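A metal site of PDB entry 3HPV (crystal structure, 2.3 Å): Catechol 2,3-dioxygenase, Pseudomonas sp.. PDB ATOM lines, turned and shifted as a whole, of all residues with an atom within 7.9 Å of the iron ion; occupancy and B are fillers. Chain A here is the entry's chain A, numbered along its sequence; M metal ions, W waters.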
ATOM      1  N   ASP A 153      -3.253  -2.441  -4.558  1.00  0.00           N
ATOM      2  CA  ASP A 153      -4.669  -2.602  -4.239  1.00  0.00           C
ATOM      3  C   ASP A 153      -5.222  -4.024  -4.310  1.00  0.00           C
ATOM      4  O   ASP A 153      -6.023  -4.434  -3.447  1.00  0.00           O
ATOM      5  CB  ASP A 153      -5.484  -1.697  -5.148  1.00  0.00           C
ATOM      6  CG  ASP A 153      -6.839  -1.408  -4.577  1.00  0.00           C
ATOM      7  OD1 ASP A 153      -6.909  -0.540  -3.662  1.00  0.00           O
ATOM      8  OD2 ASP A 153      -7.828  -2.027  -5.024  1.00  0.00           O
ATOM      9  N   HIS A 154      -4.834  -4.745  -5.353  1.00  0.00           N
ATOM     10  CA  HIS A 154      -5.289  -6.103  -5.566  1.00  0.00           C
ATOM     11  C   HIS A 154      -4.629  -6.624  -6.832  1.00  0.00           C
ATOM     12  O   HIS A 154      -3.650  -6.051  -7.307  1.00  0.00           O
ATOM     13  CB  HIS A 154      -6.822  -6.134  -5.760  1.00  0.00           C
ATOM     14  CG  HIS A 154      -7.293  -5.328  -6.930  1.00  0.00           C
ATOM     15  ND1 HIS A 154      -7.538  -3.970  -6.864  1.00  0.00           N
ATOM     16  CD2 HIS A 154      -7.508  -5.679  -8.227  1.00  0.00           C
ATOM     17  CE1 HIS A 154      -7.874  -3.517  -8.062  1.00  0.00           C
ATOM     18  NE2 HIS A 154      -7.863  -4.527  -8.902  1.00  0.00           N
ATOM     19  N   CYS A 155      -5.158  -7.721  -7.340  1.00  0.00           N
ATOM     20  CA  CYS A 155      -4.700  -8.330  -8.563  1.00  0.00           C
ATOM     21  C   CYS A 155      -5.929  -9.098  -9.011  1.00  0.00           C
ATOM     22  O   CYS A 155      -6.832  -9.325  -8.210  1.00  0.00           O
ATOM     23  CB  CYS A 155      -3.508  -9.295  -8.334  1.00  0.00           C
ATOM     24  SG  CYS A 155      -3.900 -10.908  -7.505  1.00  0.00           S
ATOM     25  N   LEU A 156      -6.004  -9.415 -10.294  1.00  0.00           N
ATOM     26  CA  LEU A 156      -7.114 -10.203 -10.799  1.00  0.00           C
ATOM     27  C   LEU A 156      -6.439 -11.400 -11.467  1.00  0.00           C
ATOM     28  O   LEU A 156      -5.436 -11.253 -12.160  1.00  0.00           O
ATOM     29  CB  LEU A 156      -7.974  -9.385 -11.793  1.00  0.00           C
ATOM     30  CG  LEU A 156      -9.207 -10.171 -12.329  1.00  0.00           C
ATOM     31  CD1 LEU A 156     -10.356  -9.237 -12.726  1.00  0.00           C
ATOM     32  CD2 LEU A 156      -8.795 -10.999 -13.517  1.00  0.00           C
ATOM     33  N   TRP A 193     -15.218 -10.954  -7.329  1.00  0.00           N
ATOM     34  CA  TRP A 193     -14.436  -9.898  -6.717  1.00  0.00           C
ATOM     35  C   TRP A 193     -14.620 -10.112  -5.222  1.00  0.00           C
ATOM     36  O   TRP A 193     -15.748 -10.053  -4.714  1.00  0.00           O
ATOM     37  CB  TRP A 193     -14.952  -8.522  -7.191  1.00  0.00           C
ATOM     38  CG  TRP A 193     -14.540  -8.195  -8.605  1.00  0.00           C
ATOM     39  CD1 TRP A 193     -13.565  -7.336  -8.992  1.00  0.00           C
ATOM     40  CD2 TRP A 193     -15.035  -8.809  -9.809  1.00  0.00           C
ATOM     41  NE1 TRP A 193     -13.406  -7.355 -10.360  1.00  0.00           N
ATOM     42  CE2 TRP A 193     -14.291  -8.253 -10.886  1.00  0.00           C
ATOM     43  CE3 TRP A 193     -16.022  -9.753 -10.091  1.00  0.00           C
ATOM     44  CZ2 TRP A 193     -14.513  -8.625 -12.218  1.00  0.00           C
ATOM     45  CZ3 TRP A 193     -16.244 -10.132 -11.432  1.00  0.00           C
ATOM     46  CH2 TRP A 193     -15.485  -9.559 -12.469  1.00  0.00           C
ATOM     47  N   HIS A 201     -12.653  -4.743  -3.471  1.00  0.00           N
ATOM     48  CA  HIS A 201     -12.016  -6.049  -3.571  1.00  0.00           C
ATOM     49  C   HIS A 201     -10.505  -5.989  -3.349  1.00  0.00           C
ATOM     50  O   HIS A 201      -9.826  -5.022  -3.729  1.00  0.00           O
ATOM     51  CB  HIS A 201     -12.338  -6.751  -4.892  1.00  0.00           C
ATOM     52  CG  HIS A 201     -11.663  -6.159  -6.091  1.00  0.00           C
ATOM     53  ND1 HIS A 201     -11.775  -4.822  -6.432  1.00  0.00           N
ATOM     54  CD2 HIS A 201     -10.908  -6.729  -7.055  1.00  0.00           C
ATOM     55  CE1 HIS A 201     -11.119  -4.605  -7.555  1.00  0.00           C
ATOM     56  NE2 HIS A 201     -10.589  -5.752  -7.957  1.00  0.00           N
ATOM     57  N   ALA A 204      -9.478 -10.653  -7.191  1.00  0.00           N
ATOM     58  CA  ALA A 204     -10.550 -11.042  -8.128  1.00  0.00           C
ATOM     59  C   ALA A 204     -10.143 -12.230  -8.979  1.00  0.00           C
ATOM     60  O   ALA A 204      -8.964 -12.393  -9.309  1.00  0.00           O
ATOM     61  CB  ALA A 204     -10.916  -9.856  -9.038  1.00  0.00           C
ATOM     62  N   HIS A 215      -3.909 -11.679 -14.781  1.00  0.00           N
ATOM     63  CA  HIS A 215      -4.497 -10.679 -15.673  1.00  0.00           C
ATOM     64  C   HIS A 215      -3.824  -9.327 -15.397  1.00  0.00           C
ATOM     65  O   HIS A 215      -3.438  -8.601 -16.324  1.00  0.00           O
ATOM     66  CB  HIS A 215      -6.001 -10.530 -15.443  1.00  0.00           C
ATOM     67  CG  HIS A 215      -6.647  -9.538 -16.356  1.00  0.00           C
ATOM     68  ND1 HIS A 215      -6.975  -9.826 -17.657  1.00  0.00           N
ATOM     69  CD2 HIS A 215      -6.978  -8.238 -16.166  1.00  0.00           C
ATOM     70  CE1 HIS A 215      -7.474  -8.753 -18.243  1.00  0.00           C
ATOM     71  NE2 HIS A 215      -7.486  -7.769 -17.357  1.00  0.00           N
ATOM     72  N   HIS A 216      -3.718  -8.973 -14.131  1.00  0.00           N
ATOM     73  CA  HIS A 216      -3.055  -7.736 -13.748  1.00  0.00           C
ATOM     74  C   HIS A 216      -2.930  -7.516 -12.279  1.00  0.00           C
ATOM     75  O   HIS A 216      -3.659  -8.097 -11.480  1.00  0.00           O
ATOM     76  CB  HIS A 216      -3.783  -6.507 -14.326  1.00  0.00           C
ATOM     77  CG  HIS A 216      -5.066  -6.148 -13.617  1.00  0.00           C
ATOM     78  ND1 HIS A 216      -6.278  -6.729 -13.932  1.00  0.00           N
ATOM     79  CD2 HIS A 216      -5.342  -5.201 -12.680  1.00  0.00           C
ATOM     80  CE1 HIS A 216      -7.240  -6.165 -13.215  1.00  0.00           C
ATOM     81  NE2 HIS A 216      -6.693  -5.228 -12.457  1.00  0.00           N
ATOM     82  N   CYS A 217      -1.969  -6.680 -11.921  1.00  0.00           N
ATOM     83  CA  CYS A 217      -1.782  -6.234 -10.560  1.00  0.00           C
ATOM     84  C   CYS A 217      -2.307  -4.794 -10.620  1.00  0.00           C
ATOM     85  O   CYS A 217      -2.266  -4.128 -11.688  1.00  0.00           O
ATOM     86  CB  CYS A 217      -0.305  -6.288 -10.155  1.00  0.00           C
ATOM     87  SG  CYS A 217       0.269  -8.016  -9.804  1.00  0.00           S
ATOM     88  N   SER A 218      -2.809  -4.301  -9.496  1.00  0.00           N
ATOM     89  CA  SER A 218      -3.382  -2.976  -9.475  1.00  0.00           C
ATOM     90  C   SER A 218      -2.866  -2.077  -8.376  1.00  0.00           C
ATOM     91  O   SER A 218      -2.643  -2.517  -7.242  1.00  0.00           O
ATOM     92  CB  SER A 218      -4.916  -3.090  -9.367  1.00  0.00           C
ATOM     93  OG  SER A 218      -5.514  -1.825  -9.168  1.00  0.00           O
ATOM     94  N   PHE A 219      -2.716  -0.793  -8.720  1.00  0.00           N
ATOM     95  CA  PHE A 219      -2.252   0.223  -7.783  1.00  0.00           C
ATOM     96  C   PHE A 219      -3.222   1.400  -7.754  1.00  0.00           C
ATOM     97  O   PHE A 219      -3.662   1.916  -8.800  1.00  0.00           O
ATOM     98  CB  PHE A 219      -0.851   0.699  -8.155  1.00  0.00           C
ATOM     99  CG  PHE A 219       0.132  -0.400  -8.416  1.00  0.00           C
ATOM    100  CD1 PHE A 219       0.195  -1.004  -9.680  1.00  0.00           C
ATOM    101  CD2 PHE A 219       0.975  -0.845  -7.406  1.00  0.00           C
ATOM    102  CE1 PHE A 219       1.101  -2.046  -9.926  1.00  0.00           C
ATOM    103  CE2 PHE A 219       1.898  -1.897  -7.643  1.00  0.00           C
ATOM    104  CZ  PHE A 219       1.953  -2.496  -8.911  1.00  0.00           C
ATOM    105  N   HIS A 248     -14.269   2.001 -15.641  1.00  0.00           N
ATOM    106  CA  HIS A 248     -14.183   0.541 -15.588  1.00  0.00           C
ATOM    107  C   HIS A 248     -15.511  -0.144 -15.872  1.00  0.00           C
ATOM    108  O   HIS A 248     -15.713  -0.693 -16.954  1.00  0.00           O
ATOM    109  CB  HIS A 248     -13.669   0.122 -14.205  1.00  0.00           C
ATOM    110  CG  HIS A 248     -13.359  -1.332 -14.086  1.00  0.00           C
ATOM    111  ND1 HIS A 248     -12.789  -1.874 -12.950  1.00  0.00           N
ATOM    112  CD2 HIS A 248     -13.525  -2.356 -14.944  1.00  0.00           C
ATOM    113  CE1 HIS A 248     -12.629  -3.168 -13.124  1.00  0.00           C
ATOM    114  NE2 HIS A 248     -13.068  -3.490 -14.321  1.00  0.00           N
ATOM    115  N   THR A 251     -16.912  -2.429 -11.335  1.00  0.00           N
ATOM    116  CA  THR A 251     -16.245  -2.061 -10.079  1.00  0.00           C
ATOM    117  C   THR A 251     -16.296  -0.549  -9.720  1.00  0.00           C
ATOM    118  O   THR A 251     -15.829  -0.158  -8.644  1.00  0.00           O
ATOM    119  CB  THR A 251     -14.761  -2.569 -10.091  1.00  0.00           C
ATOM    120  OG1 THR A 251     -14.489  -3.295  -8.887  1.00  0.00           O
ATOM    121  CG2 THR A 251     -13.779  -1.417 -10.226  1.00  0.00           C
ATOM    122  N   THR A 255     -10.046   3.849 -14.378  1.00  0.00           N
ATOM    123  CA  THR A 255      -8.752   3.215 -14.562  1.00  0.00           C
ATOM    124  C   THR A 255      -8.049   3.168 -15.933  1.00  0.00           C
ATOM    125  O   THR A 255      -8.623   3.477 -16.981  1.00  0.00           O
ATOM    126  CB  THR A 255      -8.924   1.758 -14.077  1.00  0.00           C
ATOM    127  OG1 THR A 255      -7.727   1.005 -14.308  1.00  0.00           O
ATOM    128  CG2 THR A 255     -10.057   1.114 -14.818  1.00  0.00           C
ATOM    129  N   TYR A 257      -5.356   0.403 -17.981  1.00  0.00           N
ATOM    130  CA  TYR A 257      -4.674  -0.887 -18.002  1.00  0.00           C
ATOM    131  C   TYR A 257      -3.460  -0.704 -18.915  1.00  0.00           C
ATOM    132  O   TYR A 257      -3.596  -0.372 -20.074  1.00  0.00           O
ATOM    133  CB  TYR A 257      -5.563  -1.994 -18.589  1.00  0.00           C
ATOM    134  CG  TYR A 257      -6.583  -2.566 -17.635  1.00  0.00           C
ATOM    135  CD1 TYR A 257      -6.841  -1.957 -16.406  1.00  0.00           C
ATOM    136  CD2 TYR A 257      -7.303  -3.706 -17.970  1.00  0.00           C
ATOM    137  CE1 TYR A 257      -7.809  -2.472 -15.538  1.00  0.00           C
ATOM    138  CE2 TYR A 257      -8.263  -4.238 -17.113  1.00  0.00           C
ATOM    139  CZ  TYR A 257      -8.510  -3.606 -15.903  1.00  0.00           C
ATOM    140  OH  TYR A 257      -9.465  -4.121 -15.061  1.00  0.00           O
ATOM    141  N   PHE A 266      -0.604  -4.058 -15.778  1.00  0.00           N
ATOM    142  CA  PHE A 266      -0.827  -3.462 -14.459  1.00  0.00           C
ATOM    143  C   PHE A 266      -1.952  -2.433 -14.545  1.00  0.00           C
ATOM    144  O   PHE A 266      -2.360  -2.050 -15.636  1.00  0.00           O
ATOM    145  CB  PHE A 266       0.463  -2.852 -13.868  1.00  0.00           C
ATOM    146  CG  PHE A 266       1.019  -1.683 -14.638  1.00  0.00           C
ATOM    147  CD1 PHE A 266       0.713  -0.373 -14.261  1.00  0.00           C
ATOM    148  CD2 PHE A 266       1.858  -1.903 -15.732  1.00  0.00           C
ATOM    149  CE1 PHE A 266       1.244   0.729 -14.963  1.00  0.00           C
ATOM    150  CE2 PHE A 266       2.397  -0.819 -16.445  1.00  0.00           C
ATOM    151  CZ  PHE A 266       2.091   0.497 -16.061  1.00  0.00           C
ATOM    152  N   GLU A 267      -2.485  -2.035 -13.396  1.00  0.00           N
ATOM    153  CA  GLU A 267      -3.584  -1.065 -13.380  1.00  0.00           C
ATOM    154  C   GLU A 267      -3.359   0.078 -12.424  1.00  0.00           C
ATOM    155  O   GLU A 267      -2.920  -0.119 -11.305  1.00  0.00           O
ATOM    156  CB  GLU A 267      -4.906  -1.760 -13.020  1.00  0.00           C
ATOM    157  CG  GLU A 267      -5.908  -0.874 -12.298  1.00  0.00           C
ATOM    158  CD  GLU A 267      -7.242  -1.570 -12.015  1.00  0.00           C
ATOM    159  OE1 GLU A 267      -7.262  -2.545 -11.223  1.00  0.00           O
ATOM    160  OE2 GLU A 267      -8.277  -1.149 -12.583  1.00  0.00           O
ATOM    161  N   THR A 268      -3.638   1.287 -12.910  1.00  0.00           N
ATOM    162  CA  THR A 268      -3.541   2.481 -12.091  1.00  0.00           C
ATOM    163  C   THR A 268      -5.002   2.969 -12.075  1.00  0.00           C
ATOM    164  O   THR A 268      -5.577   3.207 -13.129  1.00  0.00           O
ATOM    165  CB  THR A 268      -2.610   3.551 -12.718  1.00  0.00           C
ATOM    166  OG1 THR A 268      -3.140   3.983 -13.982  1.00  0.00           O
ATOM    167  CG2 THR A 268      -1.203   2.978 -12.950  1.00  0.00           C
ATOM    168  N   PHE A 269      -5.623   3.068 -10.901  1.00  0.00           N
ATOM    169  CA  PHE A 269      -7.018   3.509 -10.820  1.00  0.00           C
ATOM    170  C   PHE A 269      -7.326   4.235  -9.507  1.00  0.00           C
ATOM    171  O   PHE A 269      -6.481   4.317  -8.608  1.00  0.00           O
ATOM    172  CB  PHE A 269      -7.958   2.318 -10.884  1.00  0.00           C
ATOM    173  CG  PHE A 269      -8.145   1.625  -9.565  1.00  0.00           C
ATOM    174  CD1 PHE A 269      -7.101   0.921  -8.971  1.00  0.00           C
ATOM    175  CD2 PHE A 269      -9.364   1.698  -8.889  1.00  0.00           C
ATOM    176  CE1 PHE A 269      -7.264   0.296  -7.719  1.00  0.00           C
ATOM    177  CE2 PHE A 269      -9.557   1.087  -7.637  1.00  0.00           C
ATOM    178  CZ  PHE A 269      -8.499   0.378  -7.052  1.00  0.00           C
ATOM    179  N   ASP A 294     -12.537  -6.773 -18.303  1.00  0.00           N
ATOM    180  CA  ASP A 294     -11.974  -8.011 -17.760  1.00  0.00           C
ATOM    181  C   ASP A 294     -12.304  -9.250 -18.522  1.00  0.00           C
ATOM    182  O   ASP A 294     -11.935 -10.363 -18.126  1.00  0.00           O
ATOM    183  CB  ASP A 294     -12.392  -8.184 -16.304  1.00  0.00           C
ATOM    184  CG  ASP A 294     -11.838  -7.097 -15.411  1.00  0.00           C
ATOM    185  OD1 ASP A 294     -10.643  -6.768 -15.576  1.00  0.00           O
ATOM    186  OD2 ASP A 294     -12.574  -6.574 -14.564  1.00  0.00           O
HETATM  187 FE    FE M   1      -8.420  -4.195 -11.096  1.00  0.00          FE
HETATM  188  O   HOH W   1     -10.572  -2.371 -10.320  1.00  0.00           O
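OG of Ser 218 lies close to OE1 of Glu 267 (2.8 Å). The backbone carbonyl oxygen of His 216 sits at hydrogen-bond distance from the backbone NH of Leu 156 (2.9 Å). The side-chain carboxylate of Asp 153 sits at hydrogen-bond distance from a ring nitrogen (ND1) of His 154 (2.7 Å). A ring nitrogen (NE2) of His 154 lies close to a ring nitrogen (NE2) of His 201 (3.1 Å). O of His 154 lies within hydrogen-bond range of N of Ser 218 (2.9 Å). The side-chain carboxylate (OE2) of Glu 267 lies within hydrogen-bond range of the side-chain hydroxyl (OG1) of Thr 255. The backbone NH (N) of Glu 267 lies within hydrogen-bond range of the backbone carbonyl oxygen (O) of Cys 217. The backbone carbonyl oxygen (O) of Glu 267 is in hydrogen-bond range of the backbone NH (N) of Phe 219 (2.7 Å).
Of the 21 residues printed, 3 come within 4 Å of the iron ion. The nearest printed residue that does not touch the iron ion is Ser 218 (4.1 Å).
The iron ion is bound by OE1 of Glu 267 (2.0 Å), NE2 of His 154 (2.3 Å) and NE2 of His 216 (2.4 Å).
Water W1 lies within hydrogen-bond range of the side-chain carboxylate of Glu 267 (3.4 Å) and a ring nitrogen (ND1) of His 248 (3.5 Å).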
